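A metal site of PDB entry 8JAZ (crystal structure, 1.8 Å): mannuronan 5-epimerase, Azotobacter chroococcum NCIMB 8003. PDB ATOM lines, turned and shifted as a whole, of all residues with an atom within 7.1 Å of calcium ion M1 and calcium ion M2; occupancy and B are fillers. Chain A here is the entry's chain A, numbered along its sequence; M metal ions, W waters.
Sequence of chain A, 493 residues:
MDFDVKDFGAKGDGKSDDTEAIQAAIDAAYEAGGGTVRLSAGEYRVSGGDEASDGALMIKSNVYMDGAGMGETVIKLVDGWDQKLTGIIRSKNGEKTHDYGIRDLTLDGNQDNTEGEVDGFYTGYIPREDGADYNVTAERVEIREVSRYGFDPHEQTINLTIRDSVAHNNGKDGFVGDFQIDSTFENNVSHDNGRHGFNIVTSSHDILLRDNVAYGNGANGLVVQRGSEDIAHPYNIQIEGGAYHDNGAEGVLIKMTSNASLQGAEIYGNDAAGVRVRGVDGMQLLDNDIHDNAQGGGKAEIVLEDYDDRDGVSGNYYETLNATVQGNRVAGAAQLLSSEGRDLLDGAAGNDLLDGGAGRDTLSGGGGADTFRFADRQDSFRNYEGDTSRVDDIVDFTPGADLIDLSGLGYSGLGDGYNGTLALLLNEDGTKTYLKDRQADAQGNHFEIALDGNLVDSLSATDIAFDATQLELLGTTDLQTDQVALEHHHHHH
Calcium ion M2 is bound by OD2 of Asp 392 (2.2 Å), OD2 of Asp 361 (2.3 Å), O of Asp 379 (2.4 Å), O of Gly 359 (2.5 Å), O of Gly 357 (2.5 Å), water W1 (2.5 Å) and OD1 of Asp 392 (2.5 Å).
Within 4 Å of calcium ion M2: Gly 357, Gly 359, Asp 361, Asp 379 and Asp 392.
O of Ala 358 is bound to calcium ion M1 (2.3 Å).
Calcium ion M1 is bound by OD2 of Asp 343.
Calcium ion M1 is bound by O of Gly 356.
O of Gly 341 is bound to calcium ion M1 (2.3 Å).
Calcium ion M1 is bound by the side-chain carboxylate (OD1) of Asp 361 (2.4 Å).
O of Ser 339 binds calcium ion M1 (2.5 Å).
The side-chain carboxylate (OD1) of Asp 343 is in hydrogen-bond range of the side-chain hydroxyl (OG) of Ser 338 (2.8 Å).
The backbone carbonyl oxygen (O) of Asp 343 is in hydrogen-bond range of the backbone NH (N) of Thr 362.
The backbone NH (N) of Gly 357 lies within hydrogen-bond range of the side-chain carboxylate (OD1) of Asp 355, 3.1 Å away.
N of Gly 359 lies within hydrogen-bond range of OE2 of Glu 340, 3.1 Å away.
The backbone NH (N) of Asn 322 is in hydrogen-bond range of the side-chain carboxylate (OD1) of Asp 343, 3.3 Å away.
The side-chain hydroxyl of Ser 380 is in hydrogen-bond range of the backbone NH of Asp 392, at 2.8 Å.
Of the 26 residues printed, 7 come within 4 Å of calcium ion M1.
Along chain A the residues within 4 Å of calcium ion M1 span positions 339 to 361.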
ATOM      1  N   ASN A 322      27.052   3.664 -23.207  1.00  0.00           N
ATOM      2  CA  ASN A 322      26.589   3.727 -24.598  1.00  0.00           C
ATOM      3  C   ASN A 322      25.092   3.424 -24.712  1.00  0.00           C
ATOM      4  O   ASN A 322      24.674   2.453 -25.350  1.00  0.00           O
ATOM      5  CB  ASN A 322      27.415   2.781 -25.478  1.00  0.00           C
ATOM      6  CG  ASN A 322      28.910   3.056 -25.379  1.00  0.00           C
ATOM      7  OD1 ASN A 322      29.706   2.138 -25.157  1.00  0.00           O
ATOM      8  ND2 ASN A 322      29.304   4.318 -25.528  1.00  0.00           N
ATOM      9  N   SER A 338      24.026   7.265 -17.340  1.00  0.00           N
ATOM     10  CA  SER A 338      25.059   6.628 -18.141  1.00  0.00           C
ATOM     11  C   SER A 338      26.402   7.249 -17.769  1.00  0.00           C
ATOM     12  O   SER A 338      26.527   7.964 -16.775  1.00  0.00           O
ATOM     13  CB  SER A 338      24.750   6.757 -19.640  1.00  0.00           C
ATOM     14  OG  SER A 338      25.416   5.750 -20.382  1.00  0.00           O
ATOM     15  N   SER A 339      27.416   6.982 -18.593  1.00  0.00           N
ATOM     16  CA  SER A 339      28.793   7.337 -18.262  1.00  0.00           C
ATOM     17  C   SER A 339      29.530   7.666 -19.557  1.00  0.00           C
ATOM     18  O   SER A 339      28.894   7.995 -20.567  1.00  0.00           O
ATOM     19  CB  SER A 339      29.454   6.196 -17.461  1.00  0.00           C
ATOM     20  OG  SER A 339      30.810   6.492 -17.186  1.00  0.00           O
ATOM     21  N   GLU A 340      30.861   7.609 -19.519  1.00  0.00           N
ATOM     22  CA  GLU A 340      31.711   8.008 -20.640  1.00  0.00           C
ATOM     23  C   GLU A 340      31.184   7.503 -21.976  1.00  0.00           C
ATOM     24  O   GLU A 340      30.670   6.385 -22.086  1.00  0.00           O
ATOM     25  CB  GLU A 340      33.146   7.516 -20.420  1.00  0.00           C
ATOM     26  CG  GLU A 340      34.235   8.112 -21.336  1.00  0.00           C
ATOM     27  CD  GLU A 340      34.291   9.644 -21.395  1.00  0.00           C
ATOM     28  OE1 GLU A 340      35.391  10.194 -21.179  1.00  0.00           O
ATOM     29  OE2 GLU A 340      33.274  10.285 -21.746  1.00  0.00           O
ATOM     30  N   GLY A 341      31.323   8.348 -22.992  1.00  0.00           N
ATOM     31  CA  GLY A 341      30.733   8.116 -24.293  1.00  0.00           C
ATOM     32  C   GLY A 341      29.525   9.015 -24.519  1.00  0.00           C
ATOM     33  O   GLY A 341      29.003   9.663 -23.606  1.00  0.00           O
ATOM     34  N   ARG A 342      29.101   9.055 -25.778  1.00  0.00           N
ATOM     35  CA  ARG A 342      27.953   9.863 -26.179  1.00  0.00           C
ATOM     36  C   ARG A 342      26.677   9.061 -25.947  1.00  0.00           C
ATOM     37  O   ARG A 342      26.526   7.963 -26.494  1.00  0.00           O
ATOM     38  CB  ARG A 342      28.077  10.290 -27.638  1.00  0.00           C
ATOM     39  CG  ARG A 342      26.786  10.812 -28.243  1.00  0.00           C
ATOM     40  CD  ARG A 342      27.072  11.761 -29.394  1.00  0.00           C
ATOM     41  NE  ARG A 342      25.857  12.255 -30.037  1.00  0.00           N
ATOM     42  CZ  ARG A 342      25.065  13.183 -29.516  1.00  0.00           C
ATOM     43  NH1 ARG A 342      25.313  13.737 -28.338  1.00  0.00           N
ATOM     44  NH2 ARG A 342      23.990  13.566 -30.192  1.00  0.00           N
ATOM     45  N   ASP A 343      25.772   9.613 -25.146  1.00  0.00           N
ATOM     46  CA  ASP A 343      24.523   8.949 -24.802  1.00  0.00           C
ATOM     47  C   ASP A 343      23.353   9.818 -25.231  1.00  0.00           C
ATOM     48  O   ASP A 343      23.378  11.045 -25.073  1.00  0.00           O
ATOM     49  CB  ASP A 343      24.422   8.674 -23.295  1.00  0.00           C
ATOM     50  CG  ASP A 343      25.534   7.760 -22.794  1.00  0.00           C
ATOM     51  OD1 ASP A 343      25.485   6.540 -23.072  1.00  0.00           O
ATOM     52  OD2 ASP A 343      26.456   8.260 -22.108  1.00  0.00           O
ATOM     53  N   LEU A 344      22.327   9.191 -25.806  1.00  0.00           N
ATOM     54  CA  LEU A 344      21.072   9.852 -26.152  1.00  0.00           C
ATOM     55  C   LEU A 344      20.005   9.348 -25.196  1.00  0.00           C
ATOM     56  O   LEU A 344      19.606   8.180 -25.264  1.00  0.00           O
ATOM     57  CB  LEU A 344      20.686   9.582 -27.605  1.00  0.00           C
ATOM     58  CG  LEU A 344      21.804   9.712 -28.645  1.00  0.00           C
ATOM     59  CD1 LEU A 344      21.269   9.395 -30.039  1.00  0.00           C
ATOM     60  CD2 LEU A 344      22.443  11.081 -28.611  1.00  0.00           C
ATOM     61  N   LEU A 345      19.529  10.221 -24.311  1.00  0.00           N
ATOM     62  CA  LEU A 345      18.597   9.860 -23.257  1.00  0.00           C
ATOM     63  C   LEU A 345      17.349  10.717 -23.395  1.00  0.00           C
ATOM     64  O   LEU A 345      17.414  11.952 -23.267  1.00  0.00           O
ATOM     65  CB  LEU A 345      19.232  10.038 -21.880  1.00  0.00           C
ATOM     66  CG  LEU A 345      20.566   9.325 -21.657  1.00  0.00           C
ATOM     67  CD1 LEU A 345      21.043   9.468 -20.221  1.00  0.00           C
ATOM     68  CD2 LEU A 345      20.450   7.847 -22.033  1.00  0.00           C
ATOM     69  N   ASP A 355      21.053  11.979 -16.558  1.00  0.00           N
ATOM     70  CA  ASP A 355      22.454  12.338 -16.377  1.00  0.00           C
ATOM     71  C   ASP A 355      23.262  11.472 -17.333  1.00  0.00           C
ATOM     72  O   ASP A 355      23.399  10.267 -17.113  1.00  0.00           O
ATOM     73  CB  ASP A 355      22.908  12.143 -14.935  1.00  0.00           C
ATOM     74  CG  ASP A 355      24.303  12.704 -14.672  1.00  0.00           C
ATOM     75  OD1 ASP A 355      24.969  13.136 -15.637  1.00  0.00           O
ATOM     76  OD2 ASP A 355      24.726  12.711 -13.500  1.00  0.00           O
ATOM     77  N   GLY A 356      23.779  12.075 -18.404  1.00  0.00           N
ATOM     78  CA  GLY A 356      24.542  11.323 -19.375  1.00  0.00           C
ATOM     79  C   GLY A 356      25.965  11.004 -18.976  1.00  0.00           C
ATOM     80  O   GLY A 356      26.623  10.214 -19.657  1.00  0.00           O
ATOM     81  N   GLY A 357      26.444  11.584 -17.871  1.00  0.00           N
ATOM     82  CA  GLY A 357      27.803  11.342 -17.435  1.00  0.00           C
ATOM     83  C   GLY A 357      28.814  12.031 -18.336  1.00  0.00           C
ATOM     84  O   GLY A 357      28.531  13.053 -18.975  1.00  0.00           O
ATOM     85  N   ALA A 358      30.009  11.458 -18.388  1.00  0.00           N
ATOM     86  CA  ALA A 358      31.060  12.005 -19.228  1.00  0.00           C
ATOM     87  C   ALA A 358      30.706  11.859 -20.706  1.00  0.00           C
ATOM     88  O   ALA A 358      29.856  11.038 -21.087  1.00  0.00           O
ATOM     89  CB  ALA A 358      32.390  11.317 -18.918  1.00  0.00           C
ATOM     90  N   GLY A 359      31.360  12.659 -21.535  1.00  0.00           N
ATOM     91  CA  GLY A 359      31.082  12.683 -22.947  1.00  0.00           C
ATOM     92  C   GLY A 359      29.987  13.681 -23.307  1.00  0.00           C
ATOM     93  O   GLY A 359      29.360  14.308 -22.455  1.00  0.00           O
ATOM     94  N   ARG A 360      29.775  13.827 -24.611  1.00  0.00           N
ATOM     95  CA  ARG A 360      28.777  14.758 -25.143  1.00  0.00           C
ATOM     96  C   ARG A 360      27.448  14.014 -25.270  1.00  0.00           C
ATOM     97  O   ARG A 360      27.331  13.087 -26.085  1.00  0.00           O
ATOM     98  CB  ARG A 360      29.230  15.330 -26.475  1.00  0.00           C
ATOM     99  CG  ARG A 360      28.274  16.338 -27.069  1.00  0.00           C
ATOM    100  CD  ARG A 360      28.828  16.962 -28.335  1.00  0.00           C
ATOM    101  NE  ARG A 360      28.768  16.058 -29.477  1.00  0.00           N
ATOM    102  CZ  ARG A 360      27.665  15.810 -30.181  1.00  0.00           C
ATOM    103  NH1 ARG A 360      26.512  16.391 -29.887  1.00  0.00           N
ATOM    104  NH2 ARG A 360      27.726  14.964 -31.199  1.00  0.00           N
ATOM    105  N   ASP A 361      26.458  14.408 -24.483  1.00  0.00           N
ATOM    106  CA  ASP A 361      25.188  13.717 -24.400  1.00  0.00           C
ATOM    107  C   ASP A 361      24.050  14.614 -24.899  1.00  0.00           C
ATOM    108  O   ASP A 361      24.133  15.835 -24.821  1.00  0.00           O
ATOM    109  CB  ASP A 361      24.888  13.274 -22.968  1.00  0.00           C
ATOM    110  CG  ASP A 361      26.052  12.523 -22.345  1.00  0.00           C
ATOM    111  OD1 ASP A 361      26.487  11.502 -22.909  1.00  0.00           O
ATOM    112  OD2 ASP A 361      26.540  12.964 -21.279  1.00  0.00           O
ATOM    113  N   THR A 362      22.997  13.979 -25.409  1.00  0.00           N
ATOM    114  CA  THR A 362      21.785  14.658 -25.835  1.00  0.00           C
ATOM    115  C   THR A 362      20.640  14.211 -24.943  1.00  0.00           C
ATOM    116  O   THR A 362      20.217  13.045 -24.996  1.00  0.00           O
ATOM    117  CB  THR A 362      21.471  14.369 -27.304  1.00  0.00           C
ATOM    118  OG1 THR A 362      22.554  14.844 -28.125  1.00  0.00           O
ATOM    119  CG2 THR A 362      20.184  15.041 -27.730  1.00  0.00           C
ATOM    120  N   LEU A 363      20.113  15.118 -24.128  1.00  0.00           N
ATOM    121  CA  LEU A 363      19.100  14.802 -23.130  1.00  0.00           C
ATOM    122  C   LEU A 363      17.788  15.494 -23.476  1.00  0.00           C
ATOM    123  O   LEU A 363      17.775  16.640 -23.933  1.00  0.00           O
ATOM    124  CB  LEU A 363      19.566  15.235 -21.737  1.00  0.00           C
ATOM    125  CG  LEU A 363      20.990  14.900 -21.309  1.00  0.00           C
ATOM    126  CD1 LEU A 363      21.375  15.700 -20.080  1.00  0.00           C
ATOM    127  CD2 LEU A 363      21.164  13.415 -21.060  1.00  0.00           C
ATOM    128  N   PHE A 374      24.071  17.327 -13.675  1.00  0.00           N
ATOM    129  CA  PHE A 374      25.439  17.387 -14.162  1.00  0.00           C
ATOM    130  C   PHE A 374      26.350  17.279 -12.945  1.00  0.00           C
ATOM    131  O   PHE A 374      26.454  18.223 -12.151  1.00  0.00           O
ATOM    132  CB  PHE A 374      25.686  18.684 -14.937  1.00  0.00           C
ATOM    133  CG  PHE A 374      24.860  18.805 -16.193  1.00  0.00           C
ATOM    134  CD1 PHE A 374      25.417  18.513 -17.430  1.00  0.00           C
ATOM    135  CD2 PHE A 374      23.539  19.201 -16.127  1.00  0.00           C
ATOM    136  CE1 PHE A 374      24.647  18.615 -18.581  1.00  0.00           C
ATOM    137  CE2 PHE A 374      22.769  19.302 -17.277  1.00  0.00           C
ATOM    138  CZ  PHE A 374      23.333  19.007 -18.502  1.00  0.00           C
ATOM    139  N   GLN A 378      33.848  18.173 -15.728  1.00  0.00           N
ATOM    140  CA  GLN A 378      34.421  17.570 -16.923  1.00  0.00           C
ATOM    141  C   GLN A 378      33.379  16.917 -17.829  1.00  0.00           C
ATOM    142  O   GLN A 378      33.725  16.513 -18.937  1.00  0.00           O
ATOM    143  CB  GLN A 378      35.451  16.505 -16.528  1.00  0.00           C
ATOM    144  CG  GLN A 378      36.323  16.863 -15.334  1.00  0.00           C
ATOM    145  CD  GLN A 378      37.533  15.964 -15.212  1.00  0.00           C
ATOM    146  OE1 GLN A 378      37.927  15.586 -14.105  1.00  0.00           O
ATOM    147  NE2 GLN A 378      38.112  15.588 -16.352  1.00  0.00           N
ATOM    148  N   ASP A 379      32.125  16.813 -17.382  1.00  0.00           N
ATOM    149  CA  ASP A 379      31.110  16.047 -18.099  1.00  0.00           C
ATOM    150  C   ASP A 379      30.456  16.819 -19.245  1.00  0.00           C
ATOM    151  O   ASP A 379      29.696  16.213 -20.009  1.00  0.00           O
ATOM    152  CB  ASP A 379      30.037  15.572 -17.130  1.00  0.00           C
ATOM    153  CG  ASP A 379      30.523  14.444 -16.236  1.00  0.00           C
ATOM    154  OD1 ASP A 379      31.680  14.013 -16.402  1.00  0.00           O
ATOM    155  OD2 ASP A 379      29.739  13.999 -15.366  1.00  0.00           O
ATOM    156  N   SER A 380      30.707  18.123 -19.372  1.00  0.00           N
ATOM    157  CA  SER A 380      30.114  18.913 -20.448  1.00  0.00           C
ATOM    158  C   SER A 380      30.963  20.163 -20.628  1.00  0.00           C
ATOM    159  O   SER A 380      31.011  21.003 -19.729  1.00  0.00           O
ATOM    160  CB  SER A 380      28.666  19.263 -20.139  1.00  0.00           C
ATOM    161  OG  SER A 380      28.046  19.924 -21.220  1.00  0.00           O
ATOM    162  N   PHE A 381      31.632  20.288 -21.774  1.00  0.00           N
ATOM    163  CA  PHE A 381      32.578  21.382 -21.932  1.00  0.00           C
ATOM    164  C   PHE A 381      32.808  21.710 -23.399  1.00  0.00           C
ATOM    165  O   PHE A 381      32.526  20.909 -24.289  1.00  0.00           O
ATOM    166  CB  PHE A 381      33.914  21.062 -21.233  1.00  0.00           C
ATOM    167  CG  PHE A 381      34.662  19.925 -21.859  1.00  0.00           C
ATOM    168  CD1 PHE A 381      35.594  20.152 -22.859  1.00  0.00           C
ATOM    169  CD2 PHE A 381      34.459  18.626 -21.427  1.00  0.00           C
ATOM    170  CE1 PHE A 381      36.286  19.097 -23.435  1.00  0.00           C
ATOM    171  CE2 PHE A 381      35.149  17.570 -21.993  1.00  0.00           C
ATOM    172  CZ  PHE A 381      36.066  17.812 -23.006  1.00  0.00           C
ATOM    173  N   ARG A 390      32.092  19.508 -26.737  1.00  0.00           N
ATOM    174  CA  ARG A 390      31.696  18.325 -25.982  1.00  0.00           C
ATOM    175  C   ARG A 390      30.618  18.749 -25.005  1.00  0.00           C
ATOM    176  O   ARG A 390      30.644  18.408 -23.808  1.00  0.00           O
ATOM    177  CB  ARG A 390      32.889  17.741 -25.234  1.00  0.00           C
ATOM    178  CG  ARG A 390      34.161  17.586 -26.069  1.00  0.00           C
ATOM    179  CD  ARG A 390      34.051  16.472 -27.098  1.00  0.00           C
ATOM    180  NE  ARG A 390      33.256  15.358 -26.602  1.00  0.00           N
ATOM    181  CZ  ARG A 390      33.727  14.120 -26.459  1.00  0.00           C
ATOM    182  NH1 ARG A 390      34.980  13.819 -26.737  1.00  0.00           N
ATOM    183  NH2 ARG A 390      32.907  13.166 -26.018  1.00  0.00           N
ATOM    184  N   VAL A 391      29.680  19.558 -25.498  1.00  0.00           N
ATOM    185  CA  VAL A 391      28.668  20.218 -24.677  1.00  0.00           C
ATOM    186  C   VAL A 391      27.382  19.411 -24.730  1.00  0.00           C
ATOM    187  O   VAL A 391      26.803  19.208 -25.815  1.00  0.00           O
ATOM    188  CB  VAL A 391      28.429  21.655 -25.149  1.00  0.00           C
ATOM    189  CG1 VAL A 391      27.228  22.264 -24.426  1.00  0.00           C
ATOM    190  CG2 VAL A 391      29.667  22.501 -24.936  1.00  0.00           C
ATOM    191  N   ASP A 392      26.935  18.933 -23.570  1.00  0.00           N
ATOM    192  CA  ASP A 392      25.628  18.302 -23.497  1.00  0.00           C
ATOM    193  C   ASP A 392      24.548  19.300 -23.873  1.00  0.00           C
ATOM    194  O   ASP A 392      24.556  20.453 -23.428  1.00  0.00           O
ATOM    195  CB  ASP A 392      25.374  17.771 -22.077  1.00  0.00           C
ATOM    196  CG  ASP A 392      26.163  16.518 -21.772  1.00  0.00           C
ATOM    197  OD1 ASP A 392      27.058  16.155 -22.578  1.00  0.00           O
ATOM    198  OD2 ASP A 392      25.898  15.895 -20.723  1.00  0.00           O
HETATM  199 CA    CA M   1      27.871  10.020 -21.599  1.00  0.00          CA
HETATM  200 CA    CA M   2      27.813  14.768 -20.601  1.00  0.00          CA
HETATM  201  O   HOH W   1      26.797  15.267 -18.366  1.00  0.00           O
